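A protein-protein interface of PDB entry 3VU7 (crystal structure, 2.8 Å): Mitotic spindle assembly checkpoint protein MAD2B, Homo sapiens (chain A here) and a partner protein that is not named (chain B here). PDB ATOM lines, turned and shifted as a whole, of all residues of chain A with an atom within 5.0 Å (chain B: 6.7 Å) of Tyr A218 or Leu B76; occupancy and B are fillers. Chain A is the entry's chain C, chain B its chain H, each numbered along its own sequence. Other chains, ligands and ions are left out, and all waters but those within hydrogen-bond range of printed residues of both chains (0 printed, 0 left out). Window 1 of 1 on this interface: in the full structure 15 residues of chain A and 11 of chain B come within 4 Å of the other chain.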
ATOM      1  N   LYS A  98       0.942  23.439 -13.403  1.00  0.00           N
ATOM      2  CA  LYS A  98       2.238  22.887 -12.954  1.00  0.00           C
ATOM      3  C   LYS A  98       2.506  23.200 -11.498  1.00  0.00           C
ATOM      4  O   LYS A  98       2.039  24.234 -10.979  1.00  0.00           O
ATOM      5  CB  LYS A  98       3.457  23.269 -13.839  1.00  0.00           C
ATOM      6  CG  LYS A  98       3.533  24.717 -14.294  1.00  0.00           C
ATOM      7  CD  LYS A  98       4.892  25.040 -14.883  1.00  0.00           C
ATOM      8  CE  LYS A  98       4.818  25.958 -16.083  1.00  0.00           C
ATOM      9  NZ  LYS A  98       4.649  25.093 -17.279  1.00  0.00           N
ATOM     10  N   LYS A 113      14.709  25.058 -11.094  1.00  0.00           N
ATOM     11  CA  LYS A 113      13.314  24.761 -10.839  1.00  0.00           C
ATOM     12  C   LYS A 113      13.050  23.309 -11.218  1.00  0.00           C
ATOM     13  O   LYS A 113      13.491  22.875 -12.302  1.00  0.00           O
ATOM     14  CB  LYS A 113      12.409  25.655 -11.725  1.00  0.00           C
ATOM     15  CG  LYS A 113      12.576  27.171 -11.590  1.00  0.00           C
ATOM     16  CD  LYS A 113      11.776  27.862 -12.660  1.00  0.00           C
ATOM     17  CE  LYS A 113      11.859  29.371 -12.586  1.00  0.00           C
ATOM     18  NZ  LYS A 113      10.497  29.947 -12.830  1.00  0.00           N
ATOM     19  N   PHE A 114      12.345  22.570 -10.353  1.00  0.00           N
ATOM     20  CA  PHE A 114      11.858  21.244 -10.718  1.00  0.00           C
ATOM     21  C   PHE A 114      10.393  21.323 -11.060  1.00  0.00           C
ATOM     22  O   PHE A 114       9.492  21.441 -10.155  1.00  0.00           O
ATOM     23  CB  PHE A 114      12.103  20.209  -9.654  1.00  0.00           C
ATOM     24  CG  PHE A 114      13.541  19.901  -9.468  1.00  0.00           C
ATOM     25  CD1 PHE A 114      14.433  20.889  -8.984  1.00  0.00           C
ATOM     26  CD2 PHE A 114      14.030  18.664  -9.804  1.00  0.00           C
ATOM     27  CE1 PHE A 114      15.778  20.629  -8.800  1.00  0.00           C
ATOM     28  CE2 PHE A 114      15.381  18.398  -9.644  1.00  0.00           C
ATOM     29  CZ  PHE A 114      16.258  19.376  -9.129  1.00  0.00           C
ATOM     30  N   VAL A 115      10.158  21.256 -12.380  1.00  0.00           N
ATOM     31  CA  VAL A 115       8.831  21.462 -12.923  1.00  0.00           C
ATOM     32  C   VAL A 115       8.053  20.169 -13.145  1.00  0.00           C
ATOM     33  O   VAL A 115       8.443  19.333 -13.940  1.00  0.00           O
ATOM     34  CB  VAL A 115       8.900  22.302 -14.194  1.00  0.00           C
ATOM     35  CG1 VAL A 115       7.494  22.615 -14.700  1.00  0.00           C
ATOM     36  CG2 VAL A 115       9.730  23.557 -13.927  1.00  0.00           C
ATOM     37  N   GLU A 117       4.915  19.356 -14.673  1.00  0.00           N
ATOM     38  CA  GLU A 117       3.750  19.705 -15.537  1.00  0.00           C
ATOM     39  C   GLU A 117       2.686  18.605 -15.452  1.00  0.00           C
ATOM     40  O   GLU A 117       3.006  17.411 -15.556  1.00  0.00           O
ATOM     41  CB  GLU A 117       4.188  19.880 -16.992  1.00  0.00           C
ATOM     42  CG  GLU A 117       3.616  21.102 -17.665  1.00  0.00           C
ATOM     43  CD  GLU A 117       4.134  21.312 -19.086  1.00  0.00           C
ATOM     44  OE1 GLU A 117       4.229  22.498 -19.518  1.00  0.00           O
ATOM     45  OE2 GLU A 117       4.445  20.294 -19.767  1.00  0.00           O
ATOM     46  N   LEU A 202      17.240  23.275 -20.497  1.00  0.00           N
ATOM     47  CA  LEU A 202      16.188  22.370 -20.105  1.00  0.00           C
ATOM     48  C   LEU A 202      16.701  20.957 -19.969  1.00  0.00           C
ATOM     49  O   LEU A 202      17.380  20.440 -20.887  1.00  0.00           O
ATOM     50  CB  LEU A 202      15.108  22.437 -21.143  1.00  0.00           C
ATOM     51  CG  LEU A 202      13.721  22.100 -20.678  1.00  0.00           C
ATOM     52  CD1 LEU A 202      12.747  22.739 -21.649  1.00  0.00           C
ATOM     53  CD2 LEU A 202      13.571  20.595 -20.704  1.00  0.00           C
ATOM     54  N   ILE A 203      16.399  20.340 -18.820  1.00  0.00           N
ATOM     55  CA  ILE A 203      16.799  18.961 -18.587  1.00  0.00           C
ATOM     56  C   ILE A 203      15.616  18.085 -18.202  1.00  0.00           C
ATOM     57  O   ILE A 203      15.302  17.913 -17.032  1.00  0.00           O
ATOM     58  CB  ILE A 203      17.902  18.827 -17.525  1.00  0.00           C
ATOM     59  CG1 ILE A 203      19.094  19.737 -17.839  1.00  0.00           C
ATOM     60  CG2 ILE A 203      18.358  17.385 -17.419  1.00  0.00           C
ATOM     61  CD1 ILE A 203      18.980  21.127 -17.221  1.00  0.00           C
ATOM     62  N   PRO A 204      14.956  17.485 -19.195  1.00  0.00           N
ATOM     63  CA  PRO A 204      13.807  16.611 -18.870  1.00  0.00           C
ATOM     64  C   PRO A 204      14.262  15.446 -18.061  1.00  0.00           C
ATOM     65  O   PRO A 204      15.314  14.919 -18.351  1.00  0.00           O
ATOM     66  CB  PRO A 204      13.366  16.090 -20.224  1.00  0.00           C
ATOM     67  CG  PRO A 204      14.470  16.382 -21.153  1.00  0.00           C
ATOM     68  CD  PRO A 204      15.293  17.498 -20.621  1.00  0.00           C
ATOM     69  N   LEU A 205      13.499  15.020 -17.064  1.00  0.00           N
ATOM     70  CA  LEU A 205      13.838  13.734 -16.430  1.00  0.00           C
ATOM     71  C   LEU A 205      12.864  12.620 -16.829  1.00  0.00           C
ATOM     72  O   LEU A 205      13.292  11.525 -17.209  1.00  0.00           O
ATOM     73  CB  LEU A 205      14.026  13.810 -14.888  1.00  0.00           C
ATOM     74  CG  LEU A 205      14.714  15.000 -14.162  1.00  0.00           C
ATOM     75  CD1 LEU A 205      14.726  14.827 -12.640  1.00  0.00           C
ATOM     76  CD2 LEU A 205      16.108  15.330 -14.692  1.00  0.00           C
ATOM     77  N   THR A 207       8.645  11.479 -18.332  1.00  0.00           N
ATOM     78  CA  THR A 207       7.303  11.744 -18.826  1.00  0.00           C
ATOM     79  C   THR A 207       6.511  10.449 -18.584  1.00  0.00           C
ATOM     80  O   THR A 207       7.091   9.351 -18.509  1.00  0.00           O
ATOM     81  CB  THR A 207       7.351  12.123 -20.335  1.00  0.00           C
ATOM     82  OG1 THR A 207       8.136  13.319 -20.511  1.00  0.00           O
ATOM     83  CG2 THR A 207       5.965  12.347 -20.919  1.00  0.00           C
ATOM     84  N   GLN A 216       4.857  15.407 -16.701  1.00  0.00           N
ATOM     85  CA  GLN A 216       6.275  15.370 -16.959  1.00  0.00           C
ATOM     86  C   GLN A 216       7.036  16.221 -15.979  1.00  0.00           C
ATOM     87  O   GLN A 216       6.497  17.215 -15.477  1.00  0.00           O
ATOM     88  CB  GLN A 216       6.614  15.696 -18.392  1.00  0.00           C
ATOM     89  CG  GLN A 216       5.970  16.931 -18.925  1.00  0.00           C
ATOM     90  CD  GLN A 216       6.611  17.340 -20.236  1.00  0.00           C
ATOM     91  OE1 GLN A 216       7.352  16.556 -20.863  1.00  0.00           O
ATOM     92  NE2 GLN A 216       6.339  18.579 -20.665  1.00  0.00           N
ATOM     93  N   LEU A 217       8.250  15.755 -15.662  1.00  0.00           N
ATOM     94  CA  LEU A 217       9.185  16.435 -14.797  1.00  0.00           C
ATOM     95  C   LEU A 217      10.407  16.767 -15.598  1.00  0.00           C
ATOM     96  O   LEU A 217      11.094  15.881 -16.134  1.00  0.00           O
ATOM     97  CB  LEU A 217       9.568  15.536 -13.644  1.00  0.00           C
ATOM     98  CG  LEU A 217      10.709  16.059 -12.800  1.00  0.00           C
ATOM     99  CD1 LEU A 217      10.270  17.342 -12.124  1.00  0.00           C
ATOM    100  CD2 LEU A 217      11.153  15.006 -11.805  1.00  0.00           C
ATOM    101  N   TYR A 218      10.629  18.066 -15.730  1.00  0.00           N
ATOM    102  CA  TYR A 218      11.872  18.634 -16.295  1.00  0.00           C
ATOM    103  C   TYR A 218      12.397  19.663 -15.325  1.00  0.00           C
ATOM    104  O   TYR A 218      11.644  20.181 -14.482  1.00  0.00           O
ATOM    105  CB  TYR A 218      11.658  19.294 -17.656  1.00  0.00           C
ATOM    106  CG  TYR A 218      10.558  20.360 -17.728  1.00  0.00           C
ATOM    107  CD1 TYR A 218       9.224  19.995 -17.925  1.00  0.00           C
ATOM    108  CD2 TYR A 218      10.865  21.742 -17.662  1.00  0.00           C
ATOM    109  CE1 TYR A 218       8.234  20.953 -18.047  1.00  0.00           C
ATOM    110  CE2 TYR A 218       9.871  22.720 -17.784  1.00  0.00           C
ATOM    111  CZ  TYR A 218       8.552  22.316 -17.977  1.00  0.00           C
ATOM    112  OH  TYR A 218       7.509  23.240 -18.096  1.00  0.00           O
ATOM    113  N   VAL A 219      13.684  19.927 -15.430  1.00  0.00           N
ATOM    114  CA  VAL A 219      14.362  20.905 -14.614  1.00  0.00           C
ATOM    115  C   VAL A 219      14.675  22.035 -15.551  1.00  0.00           C
ATOM    116  O   VAL A 219      15.110  21.810 -16.680  1.00  0.00           O
ATOM    117  CB  VAL A 219      15.726  20.380 -14.133  1.00  0.00           C
ATOM    118  CG1 VAL A 219      16.371  21.358 -13.127  1.00  0.00           C
ATOM    119  CG2 VAL A 219      15.598  18.959 -13.595  1.00  0.00           C
ATOM    120  N   GLU A 220      14.440  23.247 -15.081  1.00  0.00           N
ATOM    121  CA  GLU A 220      14.888  24.449 -15.772  1.00  0.00           C
ATOM    122  C   GLU A 220      16.035  24.907 -14.917  1.00  0.00           C
ATOM    123  O   GLU A 220      15.847  25.148 -13.727  1.00  0.00           O
ATOM    124  CB  GLU A 220      13.782  25.538 -15.858  1.00  0.00           C
ATOM    125  CG  GLU A 220      12.569  25.131 -16.699  1.00  0.00           C
ATOM    126  CD  GLU A 220      11.670  26.290 -17.146  1.00  0.00           C
ATOM    127  OE1 GLU A 220      11.091  26.993 -16.265  1.00  0.00           O
ATOM    128  OE2 GLU A 220      11.501  26.467 -18.389  1.00  0.00           O
ATOM    129  N   LEU B  70       7.125  16.077 -30.964  1.00  0.00           N
ATOM    130  CA  LEU B  70       7.386  15.704 -29.584  1.00  0.00           C
ATOM    131  C   LEU B  70       7.276  16.954 -28.677  1.00  0.00           C
ATOM    132  O   LEU B  70       6.783  16.884 -27.525  1.00  0.00           O
ATOM    133  CB  LEU B  70       8.755  15.021 -29.438  1.00  0.00           C
ATOM    134  CG  LEU B  70       8.904  13.662 -30.151  1.00  0.00           C
ATOM    135  CD1 LEU B  70      10.209  13.003 -29.750  1.00  0.00           C
ATOM    136  CD2 LEU B  70       7.741  12.693 -29.910  1.00  0.00           C
ATOM    137  N   ILE B  71       7.714  18.102 -29.203  1.00  0.00           N
ATOM    138  CA  ILE B  71       7.606  19.358 -28.438  1.00  0.00           C
ATOM    139  C   ILE B  71       6.132  19.652 -28.194  1.00  0.00           C
ATOM    140  O   ILE B  71       5.707  19.725 -27.044  1.00  0.00           O
ATOM    141  CB  ILE B  71       8.305  20.555 -29.120  1.00  0.00           C
ATOM    142  CG1 ILE B  71       9.812  20.239 -29.320  1.00  0.00           C
ATOM    143  CG2 ILE B  71       8.049  21.800 -28.309  1.00  0.00           C
ATOM    144  CD1 ILE B  71      10.670  21.413 -29.740  1.00  0.00           C
ATOM    145  N   GLU B  73       3.498  17.727 -28.425  1.00  0.00           N
ATOM    146  CA  GLU B  73       2.892  16.701 -27.558  1.00  0.00           C
ATOM    147  C   GLU B  73       3.395  16.717 -26.139  1.00  0.00           C
ATOM    148  O   GLU B  73       3.144  15.787 -25.393  1.00  0.00           O
ATOM    149  CB  GLU B  73       3.138  15.316 -28.112  1.00  0.00           C
ATOM    150  CG  GLU B  73       2.333  15.064 -29.349  1.00  0.00           C
ATOM    151  CD  GLU B  73       0.840  15.038 -29.080  1.00  0.00           C
ATOM    152  OE1 GLU B  73       0.407  14.224 -28.213  1.00  0.00           O
ATOM    153  OE2 GLU B  73       0.117  15.819 -29.759  1.00  0.00           O
ATOM    154  N   LYS B  74       4.120  17.759 -25.763  1.00  0.00           N
ATOM    155  CA  LYS B  74       4.675  17.876 -24.413  1.00  0.00           C
ATOM    156  C   LYS B  74       5.399  16.580 -23.995  1.00  0.00           C
ATOM    157  O   LYS B  74       5.207  16.081 -22.888  1.00  0.00           O
ATOM    158  CB  LYS B  74       3.585  18.298 -23.413  1.00  0.00           C
ATOM    159  CG  LYS B  74       3.044  19.689 -23.670  1.00  0.00           C
ATOM    160  CD  LYS B  74       2.085  20.159 -22.584  1.00  0.00           C
ATOM    161  CE  LYS B  74       1.969  21.691 -22.579  1.00  0.00           C
ATOM    162  NZ  LYS B  74       3.276  22.456 -22.612  1.00  0.00           N
ATOM    163  N   ASP B  75       6.214  16.035 -24.895  1.00  0.00           N
ATOM    164  CA  ASP B  75       6.906  14.772 -24.628  1.00  0.00           C
ATOM    165  C   ASP B  75       8.440  14.907 -24.629  1.00  0.00           C
ATOM    166  O   ASP B  75       9.148  14.317 -25.484  1.00  0.00           O
ATOM    167  CB  ASP B  75       6.448  13.663 -25.585  1.00  0.00           C
ATOM    168  CG  ASP B  75       6.991  12.258 -25.182  1.00  0.00           C
ATOM    169  OD1 ASP B  75       7.886  12.113 -24.277  1.00  0.00           O
ATOM    170  OD2 ASP B  75       6.493  11.290 -25.807  1.00  0.00           O
ATOM    171  N   LEU B  76       8.928  15.644 -23.629  1.00  0.00           N
ATOM    172  CA  LEU B  76      10.306  16.067 -23.625  1.00  0.00           C
ATOM    173  C   LEU B  76      11.338  14.975 -23.312  1.00  0.00           C
ATOM    174  O   LEU B  76      12.478  15.046 -23.788  1.00  0.00           O
ATOM    175  CB  LEU B  76      10.486  17.257 -22.698  1.00  0.00           C
ATOM    176  CG  LEU B  76       9.585  18.455 -22.966  1.00  0.00           C
ATOM    177  CD1 LEU B  76       9.668  19.450 -21.806  1.00  0.00           C
ATOM    178  CD2 LEU B  76       9.947  19.090 -24.297  1.00  0.00           C
ATOM    179  N   GLU B  77      10.944  13.985 -22.506  1.00  0.00           N
ATOM    180  CA  GLU B  77      11.823  12.870 -22.205  1.00  0.00           C
ATOM    181  C   GLU B  77      12.196  12.200 -23.525  1.00  0.00           C
ATOM    182  O   GLU B  77      13.341  11.865 -23.766  1.00  0.00           O
ATOM    183  CB  GLU B  77      11.123  11.882 -21.275  1.00  0.00           C
ATOM    184  CG  GLU B  77      12.061  11.049 -20.397  1.00  0.00           C
ATOM    185  CD  GLU B  77      11.599   9.596 -20.183  1.00  0.00           C
ATOM    186  OE1 GLU B  77      10.410   9.332 -19.866  1.00  0.00           O
ATOM    187  OE2 GLU B  77      12.444   8.692 -20.329  1.00  0.00           O
ATOM    188  N   LYS B  78      11.230  12.039 -24.409  1.00  0.00           N
ATOM    189  CA  LYS B  78      11.505  11.335 -25.650  1.00  0.00           C
ATOM    190  C   LYS B  78      12.316  12.222 -26.584  1.00  0.00           C
ATOM    191  O   LYS B  78      13.161  11.741 -27.348  1.00  0.00           O
ATOM    192  CB  LYS B  78      10.196  10.882 -26.307  1.00  0.00           C
ATOM    193  CG  LYS B  78      10.377   9.717 -27.256  1.00  0.00           C
ATOM    194  CD  LYS B  78       9.056   9.338 -27.900  1.00  0.00           C
ATOM    195  CE  LYS B  78       8.261   8.410 -27.009  1.00  0.00           C
ATOM    196  NZ  LYS B  78       6.974   7.984 -27.633  1.00  0.00           N
ATOM    197  N   LEU B  79      12.045  13.524 -26.523  1.00  0.00           N
ATOM    198  CA  LEU B  79      12.751  14.499 -27.343  1.00  0.00           C
ATOM    199  C   LEU B  79      14.241  14.461 -27.016  1.00  0.00           C
ATOM    200  O   LEU B  79      15.096  14.671 -27.883  1.00  0.00           O
ATOM    201  CB  LEU B  79      12.237  15.889 -27.041  1.00  0.00           C
ATOM    202  CG  LEU B  79      13.052  16.884 -27.861  1.00  0.00           C
ATOM    203  CD1 LEU B  79      12.891  16.630 -29.358  1.00  0.00           C
ATOM    204  CD2 LEU B  79      12.583  18.279 -27.505  1.00  0.00           C
ATOM    205  N   ASP B  80      14.535  14.183 -25.748  1.00  0.00           N
ATOM    206  CA  ASP B  80      15.900  14.220 -25.275  1.00  0.00           C
ATOM    207  C   ASP B  80      16.613  12.905 -25.548  1.00  0.00           C
ATOM    208  O   ASP B  80      17.821  12.897 -25.799  1.00  0.00           O
ATOM    209  CB  ASP B  80      15.978  14.602 -23.803  1.00  0.00           C
ATOM    210  CG  ASP B  80      17.372  15.086 -23.392  1.00  0.00           C
ATOM    211  OD1 ASP B  80      17.749  14.889 -22.210  1.00  0.00           O
ATOM    212  OD2 ASP B  80      18.111  15.649 -24.240  1.00  0.00           O
ATOM    213  N   LEU B  81      15.881  11.801 -25.538  1.00  0.00           N
ATOM    214  CA  LEU B  81      16.556  10.543 -25.769  1.00  0.00           C
ATOM    215  C   LEU B  81      16.923  10.448 -27.245  1.00  0.00           C
ATOM    216  O   LEU B  81      17.965   9.894 -27.606  1.00  0.00           O
ATOM    217  CB  LEU B  81      15.716   9.348 -25.309  1.00  0.00           C
ATOM    218  CG  LEU B  81      15.311   9.264 -23.833  1.00  0.00           C
ATOM    219  CD1 LEU B  81      14.543   7.979 -23.564  1.00  0.00           C
ATOM    220  CD2 LEU B  81      16.482   9.404 -22.861  1.00  0.00           C
ATOM    221  N   LEU B 113      11.705  24.947 -29.195  1.00  0.00           N
ATOM    222  CA  LEU B 113      11.752  24.901 -27.723  1.00  0.00           C
ATOM    223  C   LEU B 113      11.822  26.269 -27.113  1.00  0.00           C
ATOM    224  O   LEU B 113      11.111  26.525 -26.138  1.00  0.00           O
ATOM    225  CB  LEU B 113      12.950  24.153 -27.192  1.00  0.00           C
ATOM    226  CG  LEU B 113      12.633  22.737 -26.738  1.00  0.00           C
ATOM    227  CD1 LEU B 113      13.891  22.083 -26.171  1.00  0.00           C
ATOM    228  CD2 LEU B 113      11.461  22.662 -25.764  1.00  0.00           C
ATOM    229  N   TYR B 117       8.754  26.621 -24.736  1.00  0.00           N
ATOM    230  CA  TYR B 117       9.082  26.450 -23.307  1.00  0.00           C
ATOM    231  C   TYR B 117       9.922  27.619 -22.737  1.00  0.00           C
ATOM    232  O   TYR B 117      10.037  27.744 -21.533  1.00  0.00           O
ATOM    233  CB  TYR B 117       9.729  25.074 -23.026  1.00  0.00           C
ATOM    234  CG  TYR B 117       8.742  23.920 -22.924  1.00  0.00           C
ATOM    235  CD1 TYR B 117       8.088  23.629 -21.712  1.00  0.00           C
ATOM    236  CD2 TYR B 117       8.460  23.110 -24.018  1.00  0.00           C
ATOM    237  CE1 TYR B 117       7.183  22.564 -21.608  1.00  0.00           C
ATOM    238  CE2 TYR B 117       7.560  22.042 -23.918  1.00  0.00           C
ATOM    239  CZ  TYR B 117       6.929  21.766 -22.723  1.00  0.00           C
ATOM    240  OH  TYR B 117       6.025  20.722 -22.638  1.00  0.00           O
ATOM    241  N   SER B 119      13.014  27.947 -23.192  1.00  0.00           N
ATOM    242  CA  SER B 119      14.198  27.218 -22.753  1.00  0.00           C
ATOM    243  C   SER B 119      14.852  26.495 -23.911  1.00  0.00           C
ATOM    244  O   SER B 119      14.174  25.892 -24.737  1.00  0.00           O
ATOM    245  CB  SER B 119      13.860  26.162 -21.693  1.00  0.00           C
ATOM    246  OG  SER B 119      12.627  26.407 -21.024  1.00  0.00           O
ATOM    247  N   LEU B 121      17.458  23.311 -24.838  1.00  0.00           N
ATOM    248  CA  LEU B 121      17.805  22.007 -24.232  1.00  0.00           C
ATOM    249  C   LEU B 121      19.260  21.955 -23.685  1.00  0.00           C
ATOM    250  O   LEU B 121      19.723  22.908 -23.067  1.00  0.00           O
ATOM    251  CB  LEU B 121      17.512  20.881 -25.226  1.00  0.00           C
ATOM    252  CG  LEU B 121      17.565  19.390 -24.916  1.00  0.00           C
ATOM    253  CD1 LEU B 121      16.623  18.692 -25.872  1.00  0.00           C
ATOM    254  CD2 LEU B 121      18.971  18.783 -25.099  1.00  0.00           C
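The side-chain amino group (NZ) of Lys B74 is in salt-bridge range of the side-chain carboxylate (OE1) of Glu A117 (3.2 Å). The backbone carbonyl oxygen (O) of Lys B74 sits close to the side-chain amide oxygen (OE1) of Gln A216 (3.0 Å). The backbone NH (N) of Leu B76 lies within hydrogen-bond range of the side-chain amide oxygen (OE1) of Gln A216, at 3.3 Å. OE1 of Glu B77 sits at hydrogen-bond distance from N of Thr A207, 3.2 Å away. OH of Tyr B117 lies within hydrogen-bond range of OE2 of Glu A117. NE2 of Gln A216 lies within hydrogen-bond range of OH of Tyr B117, 2.9 Å away. The side-chain hydroxyl of Ser B119 is in hydrogen-bond range of the side-chain carboxylate of Glu A220 (2.9 Å).
Along chain A the printed residues that touch a printed residue of chain B span positions 117 to 220.
Leu A202 touches Ser B119 (CD1 to CB, 3.6 Å). Leu A202 touches Leu B121. CG of Pro A204 touches O of Leu B76, at 3.6 Å. Pro A204 touches Asp B80 (CG to CB, 3.5 Å). Glu B77 touches Leu A205. OD1 of Asp B75 touches CG2 of Thr A207, at 3.9 Å. Thr A207 touches Leu B76. Tyr A218 touches Leu B76. Tyr A218 touches Tyr B117 (OH to CE1, 3.6 Å). Glu A220 touches Tyr B117.
The backbone carbonyl oxygen (O) of Leu B70 is in hydrogen-bond range of the backbone NH (N) of Asp B75. The side-chain hydroxyl (OH) of Tyr B117 lies within hydrogen-bond range of the side-chain amino group (NZ) of Lys B74, at 3.3 Å. OG of Ser B119 is in hydrogen-bond range of O of Tyr B117, 3.0 Å away. N of Lys A113 lies within hydrogen-bond range of O of Glu A220, 2.9 Å away. The side-chain carboxylate (OE2) of Glu A117 sits at hydrogen-bond distance from the side-chain amide nitrogen (NE2) of Gln A216. OG1 of Thr A207 lies within hydrogen-bond range of OE1 of Gln A216 (3.3 Å).
Of chain B, only Leu B76 (3.9 Å) and Tyr B117 (3.6 Å) come within 4 Å of Tyr A218. Printed residues of chain B within 4 Å of Glu A220: Tyr B117 (3.7 Å) and Ser B119 (2.9 Å). Printed residues of chain A within 4 Å of Ser B119: Leu A202 (3.6 Å) and Glu A220 (2.9 Å). Of the printed residues of chain A, Tyr B117 touches Glu A117 (3.3 Å), Gln A216 (2.9 Å), Tyr A218 (3.6 Å) and Glu A220 (3.7 Å). Printed residues of chain A within 4 Å of Asp B75: Thr A207. Val A115 touches none of the printed residues of chain B. Ile A203 touches none of the printed residues of chain B. The nearest residue of chain B that does not touch Tyr A218 is Ser B119 (5.6 Å). The nearest residue of chain A that does not touch Leu B76 is Leu A202 (4.2 Å). The nearest printed residue of chain A that does not touch Lys B74 is Thr A207 (4.3 Å).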
